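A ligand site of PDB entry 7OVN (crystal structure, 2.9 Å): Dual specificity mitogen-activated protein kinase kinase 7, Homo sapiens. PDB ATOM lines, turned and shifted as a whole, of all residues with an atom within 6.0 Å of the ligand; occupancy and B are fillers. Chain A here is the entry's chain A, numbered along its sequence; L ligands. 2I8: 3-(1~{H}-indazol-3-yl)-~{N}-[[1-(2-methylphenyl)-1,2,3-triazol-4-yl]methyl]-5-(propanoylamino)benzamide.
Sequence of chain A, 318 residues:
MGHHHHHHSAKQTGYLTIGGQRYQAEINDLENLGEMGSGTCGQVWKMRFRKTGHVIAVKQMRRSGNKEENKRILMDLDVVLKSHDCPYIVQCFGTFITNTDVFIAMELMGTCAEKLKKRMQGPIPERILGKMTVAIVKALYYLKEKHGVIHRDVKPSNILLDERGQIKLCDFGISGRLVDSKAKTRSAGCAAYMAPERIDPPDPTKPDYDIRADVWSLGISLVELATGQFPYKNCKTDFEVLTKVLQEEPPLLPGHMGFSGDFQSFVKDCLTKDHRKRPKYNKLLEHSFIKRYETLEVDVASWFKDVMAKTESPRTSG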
ATOM      1  N   MET A  36      22.475  -5.224 -14.988  1.00  0.00           N
ATOM      2  CA  MET A  36      22.658  -4.554 -16.272  1.00  0.00           C
ATOM      3  C   MET A  36      21.344  -3.900 -16.702  1.00  0.00           C
ATOM      4  O   MET A  36      20.382  -3.828 -15.939  1.00  0.00           O
ATOM      5  CB  MET A  36      23.201  -5.540 -17.314  1.00  0.00           C
ATOM      6  CG  MET A  36      24.484  -6.235 -16.870  1.00  0.00           C
ATOM      7  SD  MET A  36      25.308  -7.103 -18.212  1.00  0.00           S
ATOM      8  CE  MET A  36      23.926  -7.963 -18.945  1.00  0.00           C
ATOM      9  N   GLY A  37      21.315  -3.428 -17.948  1.00  0.00           N
ATOM     10  CA  GLY A  37      20.266  -2.522 -18.377  1.00  0.00           C
ATOM     11  C   GLY A  37      19.031  -3.103 -19.025  1.00  0.00           C
ATOM     12  O   GLY A  37      18.448  -2.491 -19.911  1.00  0.00           O
ATOM     13  N   SER A  38      18.600  -4.285 -18.575  1.00  0.00           N
ATOM     14  CA  SER A  38      17.393  -4.918 -19.101  1.00  0.00           C
ATOM     15  C   SER A  38      16.528  -5.378 -17.933  1.00  0.00           C
ATOM     16  O   SER A  38      16.880  -6.329 -17.235  1.00  0.00           O
ATOM     17  CB  SER A  38      17.751  -6.105 -20.010  1.00  0.00           C
ATOM     18  OG  SER A  38      18.693  -5.740 -20.989  1.00  0.00           O
ATOM     19  N   VAL A  44      19.140  -9.884 -15.315  1.00  0.00           N
ATOM     20  CA  VAL A  44      20.383 -10.223 -15.993  1.00  0.00           C
ATOM     21  C   VAL A  44      21.543  -9.600 -15.221  1.00  0.00           C
ATOM     22  O   VAL A  44      21.501  -8.410 -14.896  1.00  0.00           O
ATOM     23  CB  VAL A  44      20.397  -9.748 -17.457  1.00  0.00           C
ATOM     24  CG1 VAL A  44      21.521 -10.423 -18.208  1.00  0.00           C
ATOM     25  CG2 VAL A  44      19.053 -10.029 -18.125  1.00  0.00           C
ATOM     26  N   LYS A  46      25.939  -9.107 -14.791  1.00  0.00           N
ATOM     27  CA  LYS A  46      27.283  -9.191 -15.321  1.00  0.00           C
ATOM     28  C   LYS A  46      28.112 -10.020 -14.346  1.00  0.00           C
ATOM     29  O   LYS A  46      28.219  -9.664 -13.170  1.00  0.00           O
ATOM     30  CB  LYS A  46      27.875  -7.797 -15.515  1.00  0.00           C
ATOM     31  CG  LYS A  46      29.249  -7.753 -16.166  1.00  0.00           C
ATOM     32  CD  LYS A  46      29.711  -6.307 -16.331  1.00  0.00           C
ATOM     33  CE  LYS A  46      31.202  -6.210 -16.602  1.00  0.00           C
ATOM     34  NZ  LYS A  46      31.724  -4.844 -16.316  1.00  0.00           N
ATOM     35  N   VAL A  55      34.206 -12.491 -18.541  1.00  0.00           N
ATOM     36  CA  VAL A  55      33.072 -11.721 -18.041  1.00  0.00           C
ATOM     37  C   VAL A  55      31.882 -12.016 -18.950  1.00  0.00           C
ATOM     38  O   VAL A  55      31.965 -11.832 -20.170  1.00  0.00           O
ATOM     39  CB  VAL A  55      33.381 -10.219 -17.994  1.00  0.00           C
ATOM     40  CG1 VAL A  55      32.275  -9.485 -17.268  1.00  0.00           C
ATOM     41  CG2 VAL A  55      34.719  -9.979 -17.310  1.00  0.00           C
ATOM     42  N   ALA A  57      27.292 -12.470 -19.341  1.00  0.00           N
ATOM     43  CA  ALA A  57      25.959 -12.075 -18.922  1.00  0.00           C
ATOM     44  C   ALA A  57      25.184 -13.307 -18.498  1.00  0.00           C
ATOM     45  O   ALA A  57      25.221 -14.349 -19.169  1.00  0.00           O
ATOM     46  CB  ALA A  57      25.218 -11.355 -20.056  1.00  0.00           C
ATOM     47  N   LYS A  59      21.390 -14.634 -17.027  1.00  0.00           N
ATOM     48  CA  LYS A  59      19.989 -14.454 -16.698  1.00  0.00           C
ATOM     49  C   LYS A  59      19.623 -15.370 -15.540  1.00  0.00           C
ATOM     50  O   LYS A  59      19.879 -16.571 -15.608  1.00  0.00           O
ATOM     51  CB  LYS A  59      19.095 -14.751 -17.893  1.00  0.00           C
ATOM     52  CG  LYS A  59      19.229 -13.788 -19.038  1.00  0.00           C
ATOM     53  CD  LYS A  59      18.197 -14.110 -20.108  1.00  0.00           C
ATOM     54  CE  LYS A  59      18.111 -12.989 -21.115  1.00  0.00           C
ATOM     55  NZ  LYS A  59      17.075 -13.253 -22.138  1.00  0.00           N
ATOM     56  N   VAL A  90      22.817 -13.753 -30.432  1.00  0.00           N
ATOM     57  CA  VAL A  90      23.618 -13.872 -29.224  1.00  0.00           C
ATOM     58  C   VAL A  90      23.626 -15.319 -28.756  1.00  0.00           C
ATOM     59  O   VAL A  90      22.614 -16.019 -28.830  1.00  0.00           O
ATOM     60  CB  VAL A  90      23.112 -12.923 -28.120  1.00  0.00           C
ATOM     61  CG1 VAL A  90      23.097 -11.496 -28.625  1.00  0.00           C
ATOM     62  CG2 VAL A  90      21.737 -13.337 -27.641  1.00  0.00           C
ATOM     63  N   MET A 106      24.944 -16.040 -21.137  1.00  0.00           N
ATOM     64  CA  MET A 106      24.990 -15.531 -22.498  1.00  0.00           C
ATOM     65  C   MET A 106      26.243 -14.674 -22.668  1.00  0.00           C
ATOM     66  O   MET A 106      26.819 -14.184 -21.703  1.00  0.00           O
ATOM     67  CB  MET A 106      23.737 -14.696 -22.807  1.00  0.00           C
ATOM     68  CG  MET A 106      22.440 -15.374 -22.415  1.00  0.00           C
ATOM     69  SD  MET A 106      21.754 -16.411 -23.717  1.00  0.00           S
ATOM     70  CE  MET A 106      20.875 -15.177 -24.674  1.00  0.00           C
ATOM     71  N   GLU A 107      26.651 -14.507 -23.925  1.00  0.00           N
ATOM     72  CA  GLU A 107      27.823 -13.687 -24.198  1.00  0.00           C
ATOM     73  C   GLU A 107      27.536 -12.230 -23.844  1.00  0.00           C
ATOM     74  O   GLU A 107      26.407 -11.750 -23.969  1.00  0.00           O
ATOM     75  CB  GLU A 107      28.255 -13.802 -25.661  1.00  0.00           C
ATOM     76  CG  GLU A 107      27.258 -13.261 -26.664  1.00  0.00           C
ATOM     77  CD  GLU A 107      27.754 -13.430 -28.095  1.00  0.00           C
ATOM     78  OE1 GLU A 107      28.974 -13.580 -28.285  1.00  0.00           O
ATOM     79  OE2 GLU A 107      26.913 -13.416 -29.009  1.00  0.00           O
ATOM     80  N   LEU A 108      28.571 -11.540 -23.379  1.00  0.00           N
ATOM     81  CA  LEU A 108      28.454 -10.156 -22.948  1.00  0.00           C
ATOM     82  C   LEU A 108      28.783  -9.236 -24.111  1.00  0.00           C
ATOM     83  O   LEU A 108      29.809  -9.406 -24.776  1.00  0.00           O
ATOM     84  CB  LEU A 108      29.388  -9.892 -21.772  1.00  0.00           C
ATOM     85  CG  LEU A 108      29.268  -8.516 -21.106  1.00  0.00           C
ATOM     86  CD1 LEU A 108      27.892  -8.322 -20.520  1.00  0.00           C
ATOM     87  CD2 LEU A 108      30.334  -8.358 -20.042  1.00  0.00           C
ATOM     88  N   MET A 109      27.910  -8.259 -24.350  1.00  0.00           N
ATOM     89  CA  MET A 109      28.092  -7.305 -25.428  1.00  0.00           C
ATOM     90  C   MET A 109      28.055  -5.878 -24.878  1.00  0.00           C
ATOM     91  O   MET A 109      27.768  -5.648 -23.700  1.00  0.00           O
ATOM     92  CB  MET A 109      27.024  -7.484 -26.513  1.00  0.00           C
ATOM     93  CG  MET A 109      26.879  -8.915 -26.999  1.00  0.00           C
ATOM     94  SD  MET A 109      26.526  -9.014 -28.761  1.00  0.00           S
ATOM     95  CE  MET A 109      28.152  -9.402 -29.391  1.00  0.00           C
ATOM     96  N   GLY A 110      28.346  -4.923 -25.758  1.00  0.00           N
ATOM     97  CA  GLY A 110      28.451  -3.529 -25.379  1.00  0.00           C
ATOM     98  C   GLY A 110      27.157  -2.876 -24.949  1.00  0.00           C
ATOM     99  O   GLY A 110      27.032  -2.455 -23.788  1.00  0.00           O
ATOM    100  N   THR A 111      26.196  -2.766 -25.857  1.00  0.00           N
ATOM    101  CA  THR A 111      24.927  -2.125 -25.551  1.00  0.00           C
ATOM    102  C   THR A 111      23.917  -2.466 -26.643  1.00  0.00           C
ATOM    103  O   THR A 111      24.248  -3.079 -27.652  1.00  0.00           O
ATOM    104  CB  THR A 111      25.074  -0.608 -25.423  1.00  0.00           C
ATOM    105  OG1 THR A 111      23.822  -0.047 -24.999  1.00  0.00           O
ATOM    106  CG2 THR A 111      25.449   0.002 -26.768  1.00  0.00           C
ATOM    107  N   CYS A 112      22.674  -2.050 -26.409  1.00  0.00           N
ATOM    108  CA  CYS A 112      21.621  -2.156 -27.408  1.00  0.00           C
ATOM    109  C   CYS A 112      21.622  -0.909 -28.282  1.00  0.00           C
ATOM    110  O   CYS A 112      22.015   0.181 -27.844  1.00  0.00           O
ATOM    111  CB  CYS A 112      20.258  -2.345 -26.742  1.00  0.00           C
ATOM    112  SG  CYS A 112      19.621  -0.966 -25.744  1.00  0.00           S
ATOM    113  N   ALA A 113      21.201  -1.073 -29.543  1.00  0.00           N
ATOM    114  CA  ALA A 113      21.237   0.034 -30.495  1.00  0.00           C
ATOM    115  C   ALA A 113      20.428   1.227 -29.998  1.00  0.00           C
ATOM    116  O   ALA A 113      20.712   2.365 -30.372  1.00  0.00           O
ATOM    117  CB  ALA A 113      20.723  -0.423 -31.857  1.00  0.00           C
ATOM    118  N   GLU A 114      19.422   0.989 -29.152  1.00  0.00           N
ATOM    119  CA  GLU A 114      18.650   2.083 -28.572  1.00  0.00           C
ATOM    120  C   GLU A 114      19.548   2.992 -27.735  1.00  0.00           C
ATOM    121  O   GLU A 114      19.525   4.219 -27.898  1.00  0.00           O
ATOM    122  CB  GLU A 114      17.505   1.524 -27.742  1.00  0.00           C
ATOM    123  CG  GLU A 114      16.564   2.580 -27.191  1.00  0.00           C
ATOM    124  CD  GLU A 114      15.786   2.069 -25.989  1.00  0.00           C
ATOM    125  OE1 GLU A 114      16.345   1.271 -25.219  1.00  0.00           O
ATOM    126  OE2 GLU A 114      14.623   2.480 -25.814  1.00  0.00           O
ATOM    127  N   LYS A 115      20.337   2.405 -26.831  1.00  0.00           N
ATOM    128  CA  LYS A 115      21.232   3.211 -26.003  1.00  0.00           C
ATOM    129  C   LYS A 115      22.310   3.873 -26.834  1.00  0.00           C
ATOM    130  O   LYS A 115      22.734   4.988 -26.514  1.00  0.00           O
ATOM    131  CB  LYS A 115      21.855   2.344 -24.907  1.00  0.00           C
ATOM    132  CG  LYS A 115      20.856   1.744 -23.926  1.00  0.00           C
ATOM    133  CD  LYS A 115      20.243   2.800 -23.032  1.00  0.00           C
ATOM    134  CE  LYS A 115      19.120   2.226 -22.186  1.00  0.00           C
ATOM    135  NZ  LYS A 115      17.955   1.804 -23.017  1.00  0.00           N
ATOM    136  N   SER A 157      16.130  -1.839 -29.445  1.00  0.00           N
ATOM    137  CA  SER A 157      16.506  -2.463 -28.187  1.00  0.00           C
ATOM    138  C   SER A 157      16.877  -3.920 -28.345  1.00  0.00           C
ATOM    139  O   SER A 157      17.482  -4.502 -27.434  1.00  0.00           O
ATOM    140  CB  SER A 157      15.377  -2.304 -27.171  1.00  0.00           C
ATOM    141  OG  SER A 157      14.133  -2.704 -27.709  1.00  0.00           O
ATOM    142  N   ASN A 158      16.524  -4.540 -29.469  1.00  0.00           N
ATOM    143  CA  ASN A 158      16.830  -5.945 -29.733  1.00  0.00           C
ATOM    144  C   ASN A 158      17.980  -6.122 -30.711  1.00  0.00           C
ATOM    145  O   ASN A 158      18.183  -7.228 -31.231  1.00  0.00           O
ATOM    146  CB  ASN A 158      15.581  -6.672 -30.235  1.00  0.00           C
ATOM    147  CG  ASN A 158      14.509  -6.775 -29.183  1.00  0.00           C
ATOM    148  OD1 ASN A 158      14.803  -6.872 -27.991  1.00  0.00           O
ATOM    149  ND2 ASN A 158      13.252  -6.745 -29.603  1.00  0.00           N
ATOM    150  N   LEU A 160      22.083  -5.716 -30.798  1.00  0.00           N
ATOM    151  CA  LEU A 160      23.203  -5.585 -29.875  1.00  0.00           C
ATOM    152  C   LEU A 160      24.512  -5.410 -30.622  1.00  0.00           C
ATOM    153  O   LEU A 160      24.694  -5.936 -31.728  1.00  0.00           O
ATOM    154  CB  LEU A 160      23.301  -6.811 -28.955  1.00  0.00           C
ATOM    155  CG  LEU A 160      22.119  -7.078 -28.017  1.00  0.00           C
ATOM    156  CD1 LEU A 160      22.416  -8.265 -27.113  1.00  0.00           C
ATOM    157  CD2 LEU A 160      21.790  -5.849 -27.195  1.00  0.00           C
ATOM    158  N   GLU A 163      32.371  -4.469 -28.424  1.00  0.00           N
ATOM    159  CA  GLU A 163      33.643  -3.796 -28.663  1.00  0.00           C
ATOM    160  C   GLU A 163      34.330  -4.257 -29.934  1.00  0.00           C
ATOM    161  O   GLU A 163      35.228  -3.553 -30.429  1.00  0.00           O
ATOM    162  CB  GLU A 163      34.583  -4.054 -27.483  1.00  0.00           C
ATOM    163  CG  GLU A 163      34.777  -2.882 -26.534  1.00  0.00           C
ATOM    164  CD  GLU A 163      35.751  -3.203 -25.423  1.00  0.00           C
ATOM    165  OE1 GLU A 163      35.932  -4.406 -25.111  1.00  0.00           O
ATOM    166  OE2 GLU A 163      36.353  -2.264 -24.863  1.00  0.00           O
ATOM    167  N   CYS A 170      19.091  -9.860 -30.492  1.00  0.00           N
ATOM    168  CA  CYS A 170      19.132  -9.951 -29.039  1.00  0.00           C
ATOM    169  C   CYS A 170      18.395 -11.179 -28.523  1.00  0.00           C
ATOM    170  O   CYS A 170      18.875 -12.304 -28.686  1.00  0.00           O
ATOM    171  CB  CYS A 170      18.541  -8.689 -28.416  1.00  0.00           C
ATOM    172  SG  CYS A 170      18.704  -8.580 -26.625  1.00  0.00           S
ATOM    173  N   ASP A 171      17.250 -10.974 -27.889  1.00  0.00           N
ATOM    174  CA  ASP A 171      16.507 -12.062 -27.279  1.00  0.00           C
ATOM    175  C   ASP A 171      15.038 -11.978 -27.661  1.00  0.00           C
ATOM    176  O   ASP A 171      14.406 -10.930 -27.509  1.00  0.00           O
ATOM    177  CB  ASP A 171      16.692 -12.055 -25.760  1.00  0.00           C
ATOM    178  CG  ASP A 171      17.845 -12.932 -25.315  1.00  0.00           C
ATOM    179  OD1 ASP A 171      18.359 -13.692 -26.166  1.00  0.00           O
ATOM    180  OD2 ASP A 171      18.237 -12.872 -24.137  1.00  0.00           O
HETATM  181  CAB 2I8 L   1      21.731  -8.755 -23.488  1.00  0.00           C
HETATM  182  CAC 2I8 L   1      21.032  -9.887 -23.880  1.00  0.00           C
HETATM  183  CAD 2I8 L   1      21.741 -11.051 -24.115  1.00  0.00           C
HETATM  184  CAE 2I8 L   1      23.121 -11.018 -23.955  1.00  0.00           C
HETATM  185  CAF 2I8 L   1      23.069  -8.758 -23.376  1.00  0.00           C
HETATM  186  CAG 2I8 L   1      23.735  -9.893 -23.583  1.00  0.00           C
HETATM  187  CAJ 2I8 L   1      19.720  -1.873 -24.148  1.00  0.00           C
HETATM  188  CAL 2I8 L   1      19.408  -3.333 -24.442  1.00  0.00           C
HETATM  189  CAN 2I8 L   1      27.840  -3.505 -19.999  1.00  0.00           C
HETATM  190  CAO 2I8 L   1      29.267  -4.005 -20.249  1.00  0.00           C
HETATM  191  CAP 2I8 L   1      30.339  -3.577 -19.604  1.00  0.00           C
HETATM  192  CAT 2I8 L   1      32.617  -4.081 -19.697  1.00  0.00           C
HETATM  193  CAU 2I8 L   1      32.780  -3.115 -18.709  1.00  0.00           C
HETATM  194  CAV 2I8 L   1      35.002  -4.457 -19.610  1.00  0.00           C
HETATM  195  CAW 2I8 L   1      20.457  -4.346 -23.988  1.00  0.00           C
HETATM  196  CAX 2I8 L   1      25.708  -3.700 -21.176  1.00  0.00           C
HETATM  197  CAZ 2I8 L   1      23.985  -7.886 -22.940  1.00  0.00           C
HETATM  198  CBA 2I8 L   1      22.581  -4.492 -22.914  1.00  0.00           C
HETATM  199  CBB 2I8 L   1      34.024  -2.806 -18.173  1.00  0.00           C
HETATM  200  CBC 2I8 L   1      35.152  -3.485 -18.625  1.00  0.00           C
HETATM  201  CBD 2I8 L   1      33.762  -4.762 -20.153  1.00  0.00           C
HETATM  202  CBE 2I8 L   1      33.743  -5.757 -21.130  1.00  0.00           C
HETATM  203  CBF 2I8 L   1      24.753  -4.475 -21.841  1.00  0.00           C
HETATM  204  CBG 2I8 L   1      23.856  -6.571 -22.676  1.00  0.00           C
HETATM  205  CBH 2I8 L   1      22.768  -5.850 -23.144  1.00  0.00           C
HETATM  206  CBI 2I8 L   1      23.624  -3.810 -22.305  1.00  0.00           C
HETATM  207  CBJ 2I8 L   1      24.892  -5.848 -22.065  1.00  0.00           C
HETATM  208  NAA 2I8 L   1      26.814  -4.309 -20.711  1.00  0.00           N
HETATM  209  NAH 2I8 L   1      25.020  -9.635 -23.361  1.00  0.00           N
HETATM  210  NAI 2I8 L   1      25.167  -8.484 -23.031  1.00  0.00           N
HETATM  211  NAQ 2I8 L   1      31.355  -4.268 -20.128  1.00  0.00           N
HETATM  212  NAR 2I8 L   1      30.846  -5.066 -21.025  1.00  0.00           N
HETATM  213  NAS 2I8 L   1      29.635  -4.930 -21.123  1.00  0.00           N
HETATM  214  NAY 2I8 L   1      21.544  -3.789 -23.388  1.00  0.00           N
HETATM  215  OAK 2I8 L   1      20.247  -5.543 -24.178  1.00  0.00           O
HETATM  216  OAM 2I8 L   1      25.514  -2.494 -21.015  1.00  0.00           O
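SG of Cys 112 is bonded to CAJ of the ligand, at 1.8 Å. The backbone carbonyl oxygen (O) of Glu 107 is in hydrogen-bond range of a nitrogen (NAH) of the ligand (2.6 Å). NAI of the ligand sits at hydrogen-bond distance from N of Met 109 (3.1 Å). The backbone carbonyl oxygen (O) of Met 109 sits close to a nitrogen (NAA) of the ligand (3.4 Å).
SG of Cys 112 lies close to N of Lys 115 (3.6 Å). The backbone NH (N) of Met 106 lies within hydrogen-bond range of the backbone carbonyl oxygen (O) of Ala 57, at 2.6 Å. The side-chain carboxylate (OE1) of Glu 114 lies within salt-bridge range of the side-chain amino group (NZ) of Lys 115 (2.8 Å). The backbone NH (N) of Cys 170 sits at hydrogen-bond distance from the backbone carbonyl oxygen (O) of Asn 158 (2.9 Å). O of Val 44 sits at hydrogen-bond distance from N of Met 36 (3.3 Å).
O of Gly 110 lies close to OAM of the ligand (3.2 Å). Met 36 touches the ligand. Ser 38 touches the ligand. Lys 46 touches the ligand. Ala 57 touches the ligand (CB to NAH, 3.7 Å). Met 106 touches the ligand. Leu 108 touches the ligand. CA of Thr 111 touches CBI of the ligand (3.9 Å). Lys 115 touches the ligand (CG to CAJ, 3.8 Å). O of Ser 157 touches CAL of the ligand, 3.7 Å away. Leu 160 touches the ligand. SG of Cys 170 touches CAC of the ligand, at 3.8 Å. OD2 of Asp 171 touches CAD of the ligand (3.9 Å). Hydrophobic or aromatic side chains within 4 Å of the ligand: Met 36, Ala 57, Met 106, Leu 108 and Leu 160. 16 residues have an atom within 4 Å of the ligand: Met 36, Ser 38, Lys 46, Ala 57, Met 106, Glu 107, Leu 108, Met 109, Gly 110, Thr 111, Cys 112, Lys 115, Ser 157, Leu 160, Cys 170 and Asp 171. The nearest printed residue that does not touch the ligand is Val 90 (4.2 Å).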
